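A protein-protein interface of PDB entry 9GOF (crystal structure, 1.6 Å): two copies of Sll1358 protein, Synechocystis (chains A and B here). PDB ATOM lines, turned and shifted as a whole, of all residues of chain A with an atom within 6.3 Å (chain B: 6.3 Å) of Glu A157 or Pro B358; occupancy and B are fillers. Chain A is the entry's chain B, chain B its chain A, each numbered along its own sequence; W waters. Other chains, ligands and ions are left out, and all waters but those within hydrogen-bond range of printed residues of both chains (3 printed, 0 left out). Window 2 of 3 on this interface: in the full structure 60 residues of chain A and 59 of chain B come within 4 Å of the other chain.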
ATOM      1  N   ILE A 152      24.691  -0.832 -19.101  1.00  0.00           N
ATOM      2  CA  ILE A 152      25.069  -2.235 -18.940  1.00  0.00           C
ATOM      3  C   ILE A 152      23.858  -3.147 -19.070  1.00  0.00           C
ATOM      4  O   ILE A 152      23.919  -4.195 -19.724  1.00  0.00           O
ATOM      5  CB  ILE A 152      25.780  -2.439 -17.591  1.00  0.00           C
ATOM      6  CG1 ILE A 152      27.175  -1.818 -17.645  1.00  0.00           C
ATOM      7  CG2 ILE A 152      25.842  -3.924 -17.252  1.00  0.00           C
ATOM      8  CD1 ILE A 152      27.950  -1.922 -16.328  1.00  0.00           C
ATOM      9  N   ALA A 153      22.741  -2.774 -18.438  1.00  0.00           N
ATOM     10  CA  ALA A 153      21.545  -3.608 -18.505  1.00  0.00           C
ATOM     11  C   ALA A 153      21.074  -3.816 -19.938  1.00  0.00           C
ATOM     12  O   ALA A 153      20.553  -4.887 -20.265  1.00  0.00           O
ATOM     13  CB  ALA A 153      20.422  -2.988 -17.676  1.00  0.00           C
ATOM     14  N   TRP A 154      21.238  -2.807 -20.798  1.00  0.00           N
ATOM     15  CA  TRP A 154      20.828  -2.951 -22.194  1.00  0.00           C
ATOM     16  C   TRP A 154      21.813  -3.819 -22.972  1.00  0.00           C
ATOM     17  O   TRP A 154      21.413  -4.567 -23.874  1.00  0.00           O
ATOM     18  CB  TRP A 154      20.702  -1.582 -22.861  1.00  0.00           C
ATOM     19  CG  TRP A 154      19.738  -0.599 -22.236  1.00  0.00           C
ATOM     20  CD1 TRP A 154      19.306  -0.557 -20.935  1.00  0.00           C
ATOM     21  CD2 TRP A 154      19.118   0.515 -22.897  1.00  0.00           C
ATOM     22  NE1 TRP A 154      18.450   0.512 -20.750  1.00  0.00           N
ATOM     23  CE2 TRP A 154      18.317   1.180 -21.943  1.00  0.00           C
ATOM     24  CE3 TRP A 154      19.153   1.003 -24.213  1.00  0.00           C
ATOM     25  CZ2 TRP A 154      17.567   2.309 -22.258  1.00  0.00           C
ATOM     26  CZ3 TRP A 154      18.403   2.124 -24.526  1.00  0.00           C
ATOM     27  CH2 TRP A 154      17.622   2.767 -23.554  1.00  0.00           C
ATOM     28  N   VAL A 155      23.107  -3.730 -22.648  1.00  0.00           N
ATOM     29  CA  VAL A 155      24.078  -4.612 -23.289  1.00  0.00           C
ATOM     30  C   VAL A 155      23.791  -6.057 -22.910  1.00  0.00           C
ATOM     31  O   VAL A 155      23.811  -6.953 -23.764  1.00  0.00           O
ATOM     32  CB  VAL A 155      25.518  -4.208 -22.914  1.00  0.00           C
ATOM     33  CG1 VAL A 155      26.515  -5.182 -23.547  1.00  0.00           C
ATOM     34  CG2 VAL A 155      25.807  -2.780 -23.348  1.00  0.00           C
ATOM     35  N   GLU A 156      23.504  -6.303 -21.623  1.00  0.00           N
ATOM     36  CA  GLU A 156      23.105  -7.638 -21.182  1.00  0.00           C
ATOM     37  C   GLU A 156      21.943  -8.161 -22.010  1.00  0.00           C
ATOM     38  O   GLU A 156      21.975  -9.293 -22.508  1.00  0.00           O
ATOM     39  CB  GLU A 156      22.702  -7.618 -19.706  1.00  0.00           C
ATOM     40  CG  GLU A 156      23.833  -7.374 -18.740  1.00  0.00           C
ATOM     41  CD  GLU A 156      23.383  -7.577 -17.314  1.00  0.00           C
ATOM     42  OE1 GLU A 156      22.825  -8.662 -17.014  1.00  0.00           O
ATOM     43  OE2 GLU A 156      23.571  -6.650 -16.503  1.00  0.00           O
ATOM     44  N   GLU A 157      20.896  -7.344 -22.152  1.00  0.00           N
ATOM     45  CA  GLU A 157      19.716  -7.773 -22.894  1.00  0.00           C
ATOM     46  C   GLU A 157      20.039  -7.987 -24.370  1.00  0.00           C
ATOM     47  O   GLU A 157      19.577  -8.961 -24.979  1.00  0.00           O
ATOM     48  CB  GLU A 157      18.592  -6.742 -22.735  1.00  0.00           C
ATOM     49  CG  GLU A 157      17.292  -7.162 -23.398  1.00  0.00           C
ATOM     50  CD  GLU A 157      16.136  -6.219 -23.089  1.00  0.00           C
ATOM     51  OE1 GLU A 157      16.342  -5.219 -22.368  1.00  0.00           O
ATOM     52  OE2 GLU A 157      15.013  -6.498 -23.553  1.00  0.00           O
ATOM     53  N   ASN A 158      20.842  -7.092 -24.957  1.00  0.00           N
ATOM     54  CA  ASN A 158      21.164  -7.178 -26.384  1.00  0.00           C
ATOM     55  C   ASN A 158      22.007  -8.408 -26.700  1.00  0.00           C
ATOM     56  O   ASN A 158      21.864  -9.000 -27.775  1.00  0.00           O
ATOM     57  CB  ASN A 158      21.896  -5.907 -26.827  1.00  0.00           C
ATOM     58  CG  ASN A 158      21.713  -5.589 -28.309  1.00  0.00           C
ATOM     59  OD1 ASN A 158      21.337  -4.483 -28.662  1.00  0.00           O
ATOM     60  ND2 ASN A 158      21.990  -6.556 -29.172  1.00  0.00           N
ATOM     61  N   LEU A 159      22.892  -8.803 -25.789  1.00  0.00           N
ATOM     62  CA  LEU A 159      23.797  -9.918 -26.029  1.00  0.00           C
ATOM     63  C   LEU A 159      23.312 -11.218 -25.411  1.00  0.00           C
ATOM     64  O   LEU A 159      23.900 -12.274 -25.684  1.00  0.00           O
ATOM     65  CB  LEU A 159      25.196  -9.597 -25.478  1.00  0.00           C
ATOM     66  CG  LEU A 159      25.941  -8.404 -26.084  1.00  0.00           C
ATOM     67  CD1 LEU A 159      27.331  -8.305 -25.481  1.00  0.00           C
ATOM     68  CD2 LEU A 159      26.023  -8.551 -27.595  1.00  0.00           C
ATOM     69  N   GLY A 160      22.264 -11.172 -24.595  1.00  0.00           N
ATOM     70  CA  GLY A 160      21.900 -12.343 -23.813  1.00  0.00           C
ATOM     71  C   GLY A 160      22.978 -12.734 -22.826  1.00  0.00           C
ATOM     72  O   GLY A 160      23.232 -13.928 -22.625  1.00  0.00           O
ATOM     73  N   TRP A 161      23.631 -11.750 -22.214  1.00  0.00           N
ATOM     74  CA  TRP A 161      24.767 -11.970 -21.328  1.00  0.00           C
ATOM     75  C   TRP A 161      24.421 -11.564 -19.905  1.00  0.00           C
ATOM     76  O   TRP A 161      23.552 -10.723 -19.671  1.00  0.00           O
ATOM     77  CB  TRP A 161      25.985 -11.160 -21.780  1.00  0.00           C
ATOM     78  CG  TRP A 161      26.803 -11.764 -22.878  1.00  0.00           C
ATOM     79  CD1 TRP A 161      26.438 -12.769 -23.728  1.00  0.00           C
ATOM     80  CD2 TRP A 161      28.126 -11.372 -23.258  1.00  0.00           C
ATOM     81  NE1 TRP A 161      27.464 -13.038 -24.607  1.00  0.00           N
ATOM     82  CE2 TRP A 161      28.509 -12.191 -24.343  1.00  0.00           C
ATOM     83  CE3 TRP A 161      29.027 -10.406 -22.784  1.00  0.00           C
ATOM     84  CZ2 TRP A 161      29.763 -12.084 -24.956  1.00  0.00           C
ATOM     85  CZ3 TRP A 161      30.273 -10.300 -23.391  1.00  0.00           C
ATOM     86  CH2 TRP A 161      30.627 -11.131 -24.473  1.00  0.00           C
ATOM     87  N   ASN B 218       6.858  -7.695 -30.422  1.00  0.00           N
ATOM     88  CA  ASN B 218       7.494  -6.478 -30.908  1.00  0.00           C
ATOM     89  C   ASN B 218       7.471  -6.471 -32.423  1.00  0.00           C
ATOM     90  O   ASN B 218       7.738  -7.493 -33.055  1.00  0.00           O
ATOM     91  CB  ASN B 218       8.927  -6.399 -30.394  1.00  0.00           C
ATOM     92  CG  ASN B 218       8.978  -6.529 -28.894  1.00  0.00           C
ATOM     93  OD1 ASN B 218       8.588  -5.609 -28.185  1.00  0.00           O
ATOM     94  ND2 ASN B 218       9.389  -7.691 -28.403  1.00  0.00           N
ATOM     95  N   GLU B 242       6.997  -4.088 -26.630  1.00  0.00           N
ATOM     96  CA  GLU B 242       6.369  -4.648 -25.442  1.00  0.00           C
ATOM     97  C   GLU B 242       7.204  -4.302 -24.205  1.00  0.00           C
ATOM     98  O   GLU B 242       8.389  -3.970 -24.319  1.00  0.00           O
ATOM     99  CB  GLU B 242       6.247  -6.161 -25.616  1.00  0.00           C
ATOM    100  CG  GLU B 242       5.105  -6.599 -26.557  1.00  0.00           C
ATOM    101  CD  GLU B 242       3.729  -6.178 -26.060  1.00  0.00           C
ATOM    102  OE1 GLU B 242       3.337  -6.625 -24.955  1.00  0.00           O
ATOM    103  OE2 GLU B 242       3.031  -5.416 -26.765  1.00  0.00           O
ATOM    104  N   PRO B 243       6.609  -4.356 -23.013  1.00  0.00           N
ATOM    105  CA  PRO B 243       7.360  -4.001 -21.801  1.00  0.00           C
ATOM    106  C   PRO B 243       8.640  -4.807 -21.663  1.00  0.00           C
ATOM    107  O   PRO B 243       8.640  -6.038 -21.769  1.00  0.00           O
ATOM    108  CB  PRO B 243       6.372  -4.316 -20.674  1.00  0.00           C
ATOM    109  CG  PRO B 243       5.030  -4.105 -21.302  1.00  0.00           C
ATOM    110  CD  PRO B 243       5.182  -4.598 -22.726  1.00  0.00           C
ATOM    111  N   GLY B 244       9.743  -4.103 -21.409  1.00  0.00           N
ATOM    112  CA  GLY B 244      11.018  -4.740 -21.182  1.00  0.00           C
ATOM    113  C   GLY B 244      11.815  -5.023 -22.435  1.00  0.00           C
ATOM    114  O   GLY B 244      13.003  -5.353 -22.330  1.00  0.00           O
ATOM    115  N   ALA B 245      11.206  -4.889 -23.611  1.00  0.00           N
ATOM    116  CA  ALA B 245      11.837  -5.215 -24.881  1.00  0.00           C
ATOM    117  C   ALA B 245      12.612  -4.026 -25.445  1.00  0.00           C
ATOM    118  O   ALA B 245      12.403  -2.868 -25.069  1.00  0.00           O
ATOM    119  CB  ALA B 245      10.799  -5.678 -25.905  1.00  0.00           C
ATOM    120  N   MET B 246      13.462  -4.333 -26.422  1.00  0.00           N
ATOM    121  CA  MET B 246      14.521  -3.456 -26.876  1.00  0.00           C
ATOM    122  C   MET B 246      14.528  -3.530 -28.394  1.00  0.00           C
ATOM    123  O   MET B 246      14.438  -4.634 -28.936  1.00  0.00           O
ATOM    124  CB  MET B 246      15.817  -4.033 -26.307  1.00  0.00           C
ATOM    125  CG  MET B 246      16.522  -3.271 -25.244  1.00  0.00           C
ATOM    126  SD  MET B 246      18.203  -3.886 -25.280  1.00  0.00           S
ATOM    127  CE  MET B 246      18.980  -2.837 -26.482  1.00  0.00           C
ATOM    128  N   ARG B 299      14.545   1.278 -25.786  1.00  0.00           N
ATOM    129  CA  ARG B 299      14.042   0.296 -24.841  1.00  0.00           C
ATOM    130  C   ARG B 299      12.719   0.764 -24.257  1.00  0.00           C
ATOM    131  O   ARG B 299      12.534   1.950 -23.974  1.00  0.00           O
ATOM    132  CB  ARG B 299      15.049   0.035 -23.705  1.00  0.00           C
ATOM    133  CG  ARG B 299      14.617  -1.062 -22.740  1.00  0.00           C
ATOM    134  CD  ARG B 299      15.761  -1.506 -21.819  1.00  0.00           C
ATOM    135  NE  ARG B 299      15.470  -2.775 -21.156  1.00  0.00           N
ATOM    136  CZ  ARG B 299      14.796  -2.889 -20.019  1.00  0.00           C
ATOM    137  NH1 ARG B 299      14.339  -1.826 -19.374  1.00  0.00           N
ATOM    138  NH2 ARG B 299      14.576  -4.102 -19.511  1.00  0.00           N
ATOM    139  N   SER B 356      15.348  -7.341 -28.977  1.00  0.00           N
ATOM    140  CA  SER B 356      15.790  -8.211 -27.902  1.00  0.00           C
ATOM    141  C   SER B 356      14.713  -8.234 -26.828  1.00  0.00           C
ATOM    142  O   SER B 356      13.977  -7.262 -26.640  1.00  0.00           O
ATOM    143  CB  SER B 356      17.138  -7.749 -27.325  1.00  0.00           C
ATOM    144  OG  SER B 356      18.177  -8.102 -28.226  1.00  0.00           O
ATOM    145  N   LEU B 357      14.615  -9.365 -26.136  1.00  0.00           N
ATOM    146  CA  LEU B 357      13.512  -9.595 -25.221  1.00  0.00           C
ATOM    147  C   LEU B 357      13.994  -9.599 -23.777  1.00  0.00           C
ATOM    148  O   LEU B 357      15.152  -9.934 -23.503  1.00  0.00           O
ATOM    149  CB  LEU B 357      12.832 -10.936 -25.524  1.00  0.00           C
ATOM    150  CG  LEU B 357      12.432 -11.186 -26.979  1.00  0.00           C
ATOM    151  CD1 LEU B 357      11.805 -12.560 -27.104  1.00  0.00           C
ATOM    152  CD2 LEU B 357      11.462 -10.117 -27.472  1.00  0.00           C
ATOM    153  N   PRO B 358      13.128  -9.242 -22.832  1.00  0.00           N
ATOM    154  CA  PRO B 358      13.496  -9.342 -21.418  1.00  0.00           C
ATOM    155  C   PRO B 358      13.599 -10.801 -20.993  1.00  0.00           C
ATOM    156  O   PRO B 358      13.231 -11.723 -21.719  1.00  0.00           O
ATOM    157  CB  PRO B 358      12.347  -8.632 -20.698  1.00  0.00           C
ATOM    158  CG  PRO B 358      11.177  -8.781 -21.606  1.00  0.00           C
ATOM    159  CD  PRO B 358      11.729  -8.819 -23.022  1.00  0.00           C
ATOM    160  N   THR B 359      14.091 -11.009 -19.778  1.00  0.00           N
ATOM    161  CA  THR B 359      14.236 -12.374 -19.284  1.00  0.00           C
ATOM    162  C   THR B 359      12.878 -13.068 -19.225  1.00  0.00           C
ATOM    163  O   THR B 359      11.866 -12.473 -18.841  1.00  0.00           O
ATOM    164  CB  THR B 359      14.897 -12.371 -17.909  1.00  0.00           C
ATOM    165  OG1 THR B 359      14.105 -11.595 -17.006  1.00  0.00           O
ATOM    166  CG2 THR B 359      16.295 -11.775 -18.003  1.00  0.00           C
ATOM    167  N   GLN B 360      12.857 -14.338 -19.639  1.00  0.00           N
ATOM    168  CA  GLN B 360      11.662 -15.160 -19.773  1.00  0.00           C
ATOM    169  C   GLN B 360      11.491 -16.096 -18.582  1.00  0.00           C
ATOM    170  O   GLN B 360      12.475 -16.482 -17.943  1.00  0.00           O
ATOM    171  CB  GLN B 360      11.730 -15.987 -21.063  1.00  0.00           C
ATOM    172  CG  GLN B 360      11.897 -15.185 -22.361  1.00  0.00           C
ATOM    173  CD  GLN B 360      10.781 -14.164 -22.558  1.00  0.00           C
ATOM    174  OE1 GLN B 360      11.015 -12.952 -22.645  1.00  0.00           O
ATOM    175  NE2 GLN B 360       9.549 -14.655 -22.572  1.00  0.00           N
HETATM  176  O   HOH W   1      17.775 -11.056 -24.130  1.00  0.00           O
HETATM  177  O   HOH W   2      19.017 -10.527 -27.410  1.00  0.00           O
HETATM  178  O   HOH W   3      16.177  -7.182 -19.844  1.00  0.00           O
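Of the 12 printed residues of chain B, 7 touch a printed residue of chain A.
Along chain B the printed residues that touch a printed residue of chain A span positions 244 to 358.
Of the 10 printed residues of chain A, 3 touch a printed residue of chain B.
Hydrophobic or aromatic side chains of chain A within 4 Å of the printed part of chain B: Trp A154.
Among the printed residues, 11 pairs touch across the chains.
Printed residues of chain B within 4 Å of Glu A157: Gly B244 (2.6 Å), Ala B245 (3.7 Å), Met B246 (3.5 Å), Arg B299 (2.9 Å), Ser B356 (3.3 Å), Leu B357 (3.3 Å) and Pro B358 (3.4 Å).
Printed residues of chain B within 4 Å of Asn A158: Met B246 (3.6 Å) and Ser B356 (3.6 Å).
Glu B242 touches none of the printed residues of chain A.
Printed residues of chain A within 4 Å of Met B246: Trp A154 (3.6 Å), Glu A157 (3.5 Å) and Asn A158 (3.6 Å).
Of chain A, only Glu A157 comes within 4 Å of Pro B358.
The nearest printed residue of chain A that does not touch Arg B299 is Ala A153 (5.6 Å).
No position is printed for both chains.
NH2 of Arg B299 sits at hydrogen-bond distance from O of Gly B244 (3.5 Å).
The backbone carbonyl oxygen (O) of Met B246 sits at hydrogen-bond distance from the backbone NH (N) of Ser B356 (2.9 Å).
The backbone carbonyl oxygen of Pro B358 sits close to the side-chain amide oxygen of Gln B360, 2.7 Å away.
The backbone carbonyl oxygen (O) of Gly B244 lies close to the side-chain carboxylate (OE2) of Glu A157.
The guanidinium group (NE) of Arg B299 lies within salt-bridge range of the side-chain carboxylate (OE1) of Glu A157 (2.9 Å).
O of Trp A154 sits close to SD of Met B246 (3.6 Å).
OE1 of Glu A157 sits close to SD of Met B246 (3.7 Å).
OE2 of Glu A157 sits close to O of Ser B356, 3.3 Å away.
The backbone carbonyl oxygen of Leu B357 sits close to the side-chain carboxylate of Glu A157, at 3.4 Å.
N of Pro B358 lies close to OE2 of Glu A157 (3.4 Å).
Water W2 lies within hydrogen-bond range of the side-chain hydroxyl of Ser B356 (2.7 Å), the backbone carbonyl oxygen of Glu A157 (2.9 Å) and the backbone carbonyl oxygen of Asn A158 (3.3 Å).
Water W1 bridges the backbone carbonyl oxygen (O) of Glu A157 (2.9 Å) and the backbone carbonyl oxygen (O) of Leu B357 (2.9 Å).
Water W3 lies within hydrogen-bond range of OE1 of Glu A157 (3.2 Å) and NH2 of Arg B299 (3.5 Å).
Among the printed residues, merely in contact across the chains: Trp A154 with Arg B299 (3.5 Å), Glu A157 with Ala B245 (3.7 Å), Asn A158 with Met B246 (3.6 Å) and Asn A158 with Ser B356 (3.6 Å).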
